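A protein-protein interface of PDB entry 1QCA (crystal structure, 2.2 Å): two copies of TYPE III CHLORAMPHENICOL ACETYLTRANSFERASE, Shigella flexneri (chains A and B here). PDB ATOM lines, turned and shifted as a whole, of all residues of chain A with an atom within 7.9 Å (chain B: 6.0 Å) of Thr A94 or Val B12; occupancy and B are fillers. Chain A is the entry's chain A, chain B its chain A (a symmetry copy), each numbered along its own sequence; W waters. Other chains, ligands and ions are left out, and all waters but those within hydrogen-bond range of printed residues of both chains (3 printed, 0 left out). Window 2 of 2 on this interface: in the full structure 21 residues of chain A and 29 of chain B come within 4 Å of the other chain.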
ATOM      1  N   VAL A  89     -12.912  17.164  23.203  1.00  0.00           N
ATOM      2  CA  VAL A  89     -13.820  17.015  24.335  1.00  0.00           C
ATOM      3  C   VAL A  89     -14.474  18.381  24.549  1.00  0.00           C
ATOM      4  O   VAL A  89     -13.798  19.408  24.751  1.00  0.00           O
ATOM      5  CB  VAL A  89     -13.113  16.474  25.606  1.00  0.00           C
ATOM      6  CG1 VAL A  89     -13.871  16.547  26.912  1.00  0.00           C
ATOM      7  CG2 VAL A  89     -12.712  15.007  25.428  1.00  0.00           C
ATOM      8  N   PHE A  90     -15.810  18.364  24.508  1.00  0.00           N
ATOM      9  CA  PHE A  90     -16.624  19.575  24.724  1.00  0.00           C
ATOM     10  C   PHE A  90     -16.930  19.642  26.212  1.00  0.00           C
ATOM     11  O   PHE A  90     -17.253  18.640  26.815  1.00  0.00           O
ATOM     12  CB  PHE A  90     -17.881  19.523  23.872  1.00  0.00           C
ATOM     13  CG  PHE A  90     -18.693  20.761  23.825  1.00  0.00           C
ATOM     14  CD1 PHE A  90     -18.208  21.921  23.221  1.00  0.00           C
ATOM     15  CD2 PHE A  90     -19.919  20.826  24.455  1.00  0.00           C
ATOM     16  CE1 PHE A  90     -18.980  23.090  23.218  1.00  0.00           C
ATOM     17  CE2 PHE A  90     -20.686  21.987  24.442  1.00  0.00           C
ATOM     18  CZ  PHE A  90     -20.228  23.169  23.800  1.00  0.00           C
ATOM     19  N   HIS A  91     -16.864  20.855  26.735  1.00  0.00           N
ATOM     20  CA  HIS A  91     -17.195  21.250  28.089  1.00  0.00           C
ATOM     21  C   HIS A  91     -18.521  21.990  28.034  1.00  0.00           C
ATOM     22  O   HIS A  91     -18.525  23.163  27.549  1.00  0.00           O
ATOM     23  CB  HIS A  91     -16.124  22.169  28.713  1.00  0.00           C
ATOM     24  CG  HIS A  91     -14.774  21.487  28.745  1.00  0.00           C
ATOM     25  ND1 HIS A  91     -14.481  20.301  29.335  1.00  0.00           N
ATOM     26  CD2 HIS A  91     -13.597  21.937  28.218  1.00  0.00           C
ATOM     27  CE1 HIS A  91     -13.200  19.998  29.172  1.00  0.00           C
ATOM     28  NE2 HIS A  91     -12.625  20.987  28.507  1.00  0.00           N
ATOM     29  N   GLN A  92     -19.596  21.353  28.416  1.00  0.00           N
ATOM     30  CA  GLN A  92     -20.906  22.036  28.319  1.00  0.00           C
ATOM     31  C   GLN A  92     -20.952  23.307  29.141  1.00  0.00           C
ATOM     32  O   GLN A  92     -21.624  24.297  28.849  1.00  0.00           O
ATOM     33  CB  GLN A  92     -22.067  21.130  28.740  1.00  0.00           C
ATOM     34  CG  GLN A  92     -23.218  21.201  27.693  1.00  0.00           C
ATOM     35  N   GLU A  93     -20.225  23.282  30.233  1.00  0.00           N
ATOM     36  CA  GLU A  93     -20.186  24.436  31.152  1.00  0.00           C
ATOM     37  C   GLU A  93     -19.607  25.730  30.567  1.00  0.00           C
ATOM     38  O   GLU A  93     -20.079  26.854  30.854  1.00  0.00           O
ATOM     39  CB  GLU A  93     -19.321  24.145  32.412  1.00  0.00           C
ATOM     40  CG  GLU A  93     -19.522  22.782  33.078  1.00  0.00           C
ATOM     41  CD  GLU A  93     -19.031  21.606  32.262  1.00  0.00           C
ATOM     42  OE1 GLU A  93     -17.890  21.861  31.813  1.00  0.00           O
ATOM     43  OE2 GLU A  93     -19.730  20.623  32.090  1.00  0.00           O
ATOM     44  N   THR A  94     -18.525  25.563  29.834  1.00  0.00           N
ATOM     45  CA  THR A  94     -17.868  26.762  29.297  1.00  0.00           C
ATOM     46  C   THR A  94     -18.147  26.908  27.818  1.00  0.00           C
ATOM     47  O   THR A  94     -17.839  27.953  27.292  1.00  0.00           O
ATOM     48  CB  THR A  94     -16.327  26.747  29.582  1.00  0.00           C
ATOM     49  OG1 THR A  94     -15.893  25.470  29.032  1.00  0.00           O
ATOM     50  CG2 THR A  94     -15.915  26.734  31.067  1.00  0.00           C
ATOM     51  N   GLU A  95     -18.731  25.859  27.275  1.00  0.00           N
ATOM     52  CA  GLU A  95     -19.046  25.721  25.845  1.00  0.00           C
ATOM     53  C   GLU A  95     -17.742  25.809  25.034  1.00  0.00           C
ATOM     54  O   GLU A  95     -17.717  26.468  23.960  1.00  0.00           O
ATOM     55  CB  GLU A  95     -20.098  26.707  25.306  1.00  0.00           C
ATOM     56  CG  GLU A  95     -21.449  26.450  25.996  1.00  0.00           C
ATOM     57  CD  GLU A  95     -22.550  27.352  25.487  1.00  0.00           C
ATOM     58  OE1 GLU A  95     -22.399  28.386  24.880  1.00  0.00           O
ATOM     59  OE2 GLU A  95     -23.667  26.865  25.809  1.00  0.00           O
ATOM     60  N   THR A  96     -16.702  25.214  25.602  1.00  0.00           N
ATOM     61  CA  THR A  96     -15.389  25.298  24.913  1.00  0.00           C
ATOM     62  C   THR A  96     -14.910  23.846  24.821  1.00  0.00           C
ATOM     63  O   THR A  96     -15.453  22.918  25.431  1.00  0.00           O
ATOM     64  CB  THR A  96     -14.347  26.176  25.682  1.00  0.00           C
ATOM     65  OG1 THR A  96     -14.202  25.546  27.023  1.00  0.00           O
ATOM     66  CG2 THR A  96     -14.716  27.644  25.856  1.00  0.00           C
ATOM     67  N   PHE A  97     -13.877  23.623  24.026  1.00  0.00           N
ATOM     68  CA  PHE A  97     -13.350  22.252  23.887  1.00  0.00           C
ATOM     69  C   PHE A  97     -11.876  22.236  24.313  1.00  0.00           C
ATOM     70  O   PHE A  97     -11.195  23.273  24.422  1.00  0.00           O
ATOM     71  CB  PHE A  97     -13.513  21.718  22.440  1.00  0.00           C
ATOM     72  CG  PHE A  97     -12.605  22.364  21.419  1.00  0.00           C
ATOM     73  CD1 PHE A  97     -12.853  23.601  20.801  1.00  0.00           C
ATOM     74  CD2 PHE A  97     -11.358  21.758  21.162  1.00  0.00           C
ATOM     75  CE1 PHE A  97     -11.950  24.193  19.919  1.00  0.00           C
ATOM     76  CE2 PHE A  97     -10.405  22.310  20.326  1.00  0.00           C
ATOM     77  CZ  PHE A  97     -10.738  23.516  19.636  1.00  0.00           C
ATOM     78  N   SER A  98     -11.460  20.973  24.504  1.00  0.00           N
ATOM     79  CA  SER A  98     -10.111  20.641  24.874  1.00  0.00           C
ATOM     80  C   SER A  98      -9.684  19.488  23.954  1.00  0.00           C
ATOM     81  O   SER A  98     -10.541  18.750  23.472  1.00  0.00           O
ATOM     82  CB  SER A  98     -10.010  20.194  26.326  1.00  0.00           C
ATOM     83  OG  SER A  98     -10.321  21.222  27.240  1.00  0.00           O
ATOM     84  N   SER A 124     -12.754  17.920  33.919  1.00  0.00           N
ATOM     85  CA  SER A 124     -12.962  19.272  34.434  1.00  0.00           C
ATOM     86  C   SER A 124     -12.013  20.328  33.905  1.00  0.00           C
ATOM     87  O   SER A 124     -12.280  21.526  34.108  1.00  0.00           O
ATOM     88  CB  SER A 124     -13.009  19.112  35.975  1.00  0.00           C
ATOM     89  OG  SER A 124     -14.065  18.240  36.408  1.00  0.00           O
ATOM     90  N   ASP A 125     -10.993  19.923  33.216  1.00  0.00           N
ATOM     91  CA  ASP A 125      -9.914  20.768  32.695  1.00  0.00           C
ATOM     92  C   ASP A 125     -10.197  21.477  31.365  1.00  0.00           C
ATOM     93  O   ASP A 125     -10.262  20.940  30.275  1.00  0.00           O
ATOM     94  CB  ASP A 125      -8.582  19.980  32.804  1.00  0.00           C
ATOM     95  CG  ASP A 125      -7.341  20.832  32.685  1.00  0.00           C
ATOM     96  OD1 ASP A 125      -7.244  21.952  32.136  1.00  0.00           O
ATOM     97  OD2 ASP A 125      -6.313  20.348  33.208  1.00  0.00           O
ATOM     98  N   THR A 126     -10.289  22.790  31.520  1.00  0.00           N
ATOM     99  CA  THR A 126     -10.573  23.691  30.416  1.00  0.00           C
ATOM    100  C   THR A 126      -9.365  24.167  29.634  1.00  0.00           C
ATOM    101  O   THR A 126      -9.632  24.876  28.637  1.00  0.00           O
ATOM    102  CB  THR A 126     -11.609  24.841  30.794  1.00  0.00           C
ATOM    103  OG1 THR A 126     -10.833  25.687  31.703  1.00  0.00           O
ATOM    104  CG2 THR A 126     -12.889  24.138  31.293  1.00  0.00           C
ATOM    105  N   LYS A 127      -8.145  23.781  29.988  1.00  0.00           N
ATOM    106  CA  LYS A 127      -7.061  24.212  29.118  1.00  0.00           C
ATOM    107  C   LYS A 127      -7.283  23.557  27.723  1.00  0.00           C
ATOM    108  O   LYS A 127      -7.938  22.486  27.632  1.00  0.00           O
ATOM    109  CB  LYS A 127      -5.768  23.659  29.682  1.00  0.00           C
ATOM    110  CG  LYS A 127      -5.306  24.358  30.919  1.00  0.00           C
ATOM    111  CD  LYS A 127      -4.046  23.727  31.528  1.00  0.00           C
ATOM    112  N   LEU A 128      -6.731  24.101  26.686  1.00  0.00           N
ATOM    113  CA  LEU A 128      -6.782  23.599  25.306  1.00  0.00           C
ATOM    114  C   LEU A 128      -6.077  22.216  25.260  1.00  0.00           C
ATOM    115  O   LEU A 128      -6.581  21.209  24.688  1.00  0.00           O
ATOM    116  CB  LEU A 128      -6.413  24.718  24.313  1.00  0.00           C
ATOM    117  CG  LEU A 128      -6.303  24.109  22.887  1.00  0.00           C
ATOM    118  CD1 LEU A 128      -7.587  23.510  22.260  1.00  0.00           C
ATOM    119  CD2 LEU A 128      -5.684  25.161  22.011  1.00  0.00           C
ATOM    120  N   ASN B  10     -10.713  37.759  30.436  1.00  0.00           N
ATOM    121  CA  ASN B  10     -11.556  36.873  31.315  1.00  0.00           C
ATOM    122  C   ASN B  10     -12.438  35.965  30.480  1.00  0.00           C
ATOM    123  O   ASN B  10     -13.381  35.369  31.028  1.00  0.00           O
ATOM    124  CB  ASN B  10     -12.250  37.829  32.301  1.00  0.00           C
ATOM    125  CG  ASN B  10     -11.242  38.489  33.241  1.00  0.00           C
ATOM    126  N   TRP B  11     -12.171  35.882  29.193  1.00  0.00           N
ATOM    127  CA  TRP B  11     -12.947  35.077  28.236  1.00  0.00           C
ATOM    128  C   TRP B  11     -12.551  33.615  28.386  1.00  0.00           C
ATOM    129  O   TRP B  11     -11.348  33.357  28.547  1.00  0.00           O
ATOM    130  CB  TRP B  11     -12.658  35.598  26.841  1.00  0.00           C
ATOM    131  CG  TRP B  11     -13.399  35.060  25.686  1.00  0.00           C
ATOM    132  CD1 TRP B  11     -14.642  34.460  25.655  1.00  0.00           C
ATOM    133  CD2 TRP B  11     -12.990  35.153  24.325  1.00  0.00           C
ATOM    134  NE1 TRP B  11     -15.042  34.148  24.375  1.00  0.00           N
ATOM    135  CE2 TRP B  11     -14.035  34.573  23.540  1.00  0.00           C
ATOM    136  CE3 TRP B  11     -11.872  35.668  23.702  1.00  0.00           C
ATOM    137  CZ2 TRP B  11     -13.943  34.502  22.157  1.00  0.00           C
ATOM    138  CZ3 TRP B  11     -11.798  35.607  22.317  1.00  0.00           C
ATOM    139  CH2 TRP B  11     -12.820  35.042  21.571  1.00  0.00           C
ATOM    140  N   VAL B  12     -13.548  32.746  28.333  1.00  0.00           N
ATOM    141  CA  VAL B  12     -13.223  31.322  28.458  1.00  0.00           C
ATOM    142  C   VAL B  12     -12.367  30.765  27.306  1.00  0.00           C
ATOM    143  O   VAL B  12     -11.663  29.782  27.400  1.00  0.00           O
ATOM    144  CB  VAL B  12     -14.511  30.519  28.626  1.00  0.00           C
ATOM    145  CG1 VAL B  12     -15.166  30.736  29.975  1.00  0.00           C
ATOM    146  CG2 VAL B  12     -15.563  30.763  27.563  1.00  0.00           C
ATOM    147  N   ARG B  13     -12.485  31.274  26.125  1.00  0.00           N
ATOM    148  CA  ARG B  13     -11.824  30.949  24.897  1.00  0.00           C
ATOM    149  C   ARG B  13     -10.556  31.819  24.777  1.00  0.00           C
ATOM    150  O   ARG B  13     -10.057  31.897  23.647  1.00  0.00           O
ATOM    151  CB  ARG B  13     -12.684  31.191  23.663  1.00  0.00           C
ATOM    152  CG  ARG B  13     -13.819  30.248  23.436  1.00  0.00           C
ATOM    153  CD  ARG B  13     -14.493  30.461  22.144  1.00  0.00           C
ATOM    154  NE  ARG B  13     -13.814  29.805  21.039  1.00  0.00           N
ATOM    155  CZ  ARG B  13     -12.994  30.420  20.182  1.00  0.00           C
ATOM    156  NH1 ARG B  13     -12.778  31.729  20.346  1.00  0.00           N
ATOM    157  NH2 ARG B  13     -12.441  29.688  19.202  1.00  0.00           N
ATOM    158  N   ARG B  14      -9.998  32.466  25.772  1.00  0.00           N
ATOM    159  CA  ARG B  14      -8.800  33.266  25.439  1.00  0.00           C
ATOM    160  C   ARG B  14      -7.661  32.425  24.893  1.00  0.00           C
ATOM    161  O   ARG B  14      -6.880  32.807  23.998  1.00  0.00           O
ATOM    162  CB  ARG B  14      -8.357  34.226  26.578  1.00  0.00           C
ATOM    163  CG  ARG B  14      -7.978  33.502  27.850  1.00  0.00           C
ATOM    164  N   GLU B  15      -7.471  31.218  25.363  1.00  0.00           N
ATOM    165  CA  GLU B  15      -6.309  30.450  24.840  1.00  0.00           C
ATOM    166  C   GLU B  15      -6.534  30.100  23.395  1.00  0.00           C
ATOM    167  O   GLU B  15      -5.657  30.263  22.527  1.00  0.00           O
ATOM    168  CB  GLU B  15      -6.056  29.302  25.801  1.00  0.00           C
ATOM    169  CG  GLU B  15      -4.858  28.444  25.499  1.00  0.00           C
ATOM    170  CD  GLU B  15      -4.825  27.113  26.204  1.00  0.00           C
ATOM    171  OE1 GLU B  15      -5.606  26.623  27.003  1.00  0.00           O
ATOM    172  OE2 GLU B  15      -3.818  26.425  25.851  1.00  0.00           O
ATOM    173  N   HIS B  16      -7.756  29.656  23.117  1.00  0.00           N
ATOM    174  CA  HIS B  16      -8.163  29.232  21.764  1.00  0.00           C
ATOM    175  C   HIS B  16      -7.973  30.362  20.744  1.00  0.00           C
ATOM    176  O   HIS B  16      -7.577  30.225  19.595  1.00  0.00           O
ATOM    177  CB  HIS B  16      -9.659  28.771  21.704  1.00  0.00           C
ATOM    178  CG  HIS B  16      -9.943  27.719  22.738  1.00  0.00           C
ATOM    179  ND1 HIS B  16     -10.030  27.951  24.070  1.00  0.00           N
ATOM    180  CD2 HIS B  16     -10.145  26.371  22.584  1.00  0.00           C
ATOM    181  CE1 HIS B  16     -10.280  26.797  24.684  1.00  0.00           C
ATOM    182  NE2 HIS B  16     -10.356  25.811  23.825  1.00  0.00           N
HETATM  183  O   HOH W   1     -13.181  26.439  22.721  1.00  0.00           O
HETATM  184  O   HOH W   2      -8.241  27.256  27.998  1.00  0.00           O
HETATM  185  O   HOH W   3      -3.396  24.098  26.920  1.00  0.00           O
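The backbone NH (N) of Leu A128 lies within hydrogen-bond range of the side-chain carboxylate (OE1) of Glu B15. A ring nitrogen (NE2) of His B16 lies within hydrogen-bond range of the backbone carbonyl oxygen of Phe A97, 2.7 Å away.
The backbone NH (N) of Lys A127 lies within hydrogen-bond range of the side-chain carboxylate (OD1) of Asp A125 (3.0 Å). N of His A91 lies within hydrogen-bond range of O of Thr A96 (2.8 Å). The side-chain hydroxyl (OG1) of Thr A96 is in hydrogen-bond range of the side-chain hydroxyl (OG1) of Thr A94, 2.6 Å away. The side-chain hydroxyl (OG) of Ser A98 is in hydrogen-bond range of the backbone carbonyl oxygen (O) of Lys A127 (2.7 Å).
Thr A94 touches Val B12 (O to CG2, 3.6 Å). Thr A96 touches Val B12. CG2 of Thr A96 touches CG of Arg B13, 3.7 Å away. Lys A127 touches Glu B15. Leu A128 touches His B16 (CD1 to CD2, 3.9 Å).
Of the printed residues of chain B, Thr A94 touches Val B12. Printed residues of chain A within 4 Å of Val B12: Thr A94 and Thr A96. Printed residues of chain B within 4 Å of Leu A128: Glu B15 (2.8 Å) and His B16 (3.9 Å). Of the printed residues of chain B, Phe A97 touches His B16. Printed residues of chain A within 4 Å of Glu B15: Lys A127 and Leu A128. Printed residues of chain B within 4 Å of Thr A96: Val B12 (3.7 Å) and Arg B13 (3.7 Å). The nearest residue of chain A that does not touch Val B12 is Thr A126 (5.5 Å). The nearest printed residue of chain B that does not touch Lys A127 is His B16 (5.4 Å).
Hydrophobic or aromatic side chains of chain A that line the printed part of chain B: Phe A97 and Leu A128. Among the printed residues, 7 pairs touch across the chains. Among the printed residues, no Asp or Glu carboxylate lies within 4 Å of a Lys or Arg side-chain nitrogen of the other chain.
No position is printed for both chains.
Water W3 lies within hydrogen-bond range of the side-chain carboxylate of Glu B15 and the backbone NH of Leu A128. Water W2 lies within hydrogen-bond range of the backbone carbonyl oxygen (O) of Thr A126 (2.8 Å) and the side-chain carboxylate (OE1) of Glu B15 (2.9 Å). Water W1 lies within hydrogen-bond range of NE2 of His B16 (3.1 Å) and N of Phe A97 (3.2 Å).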
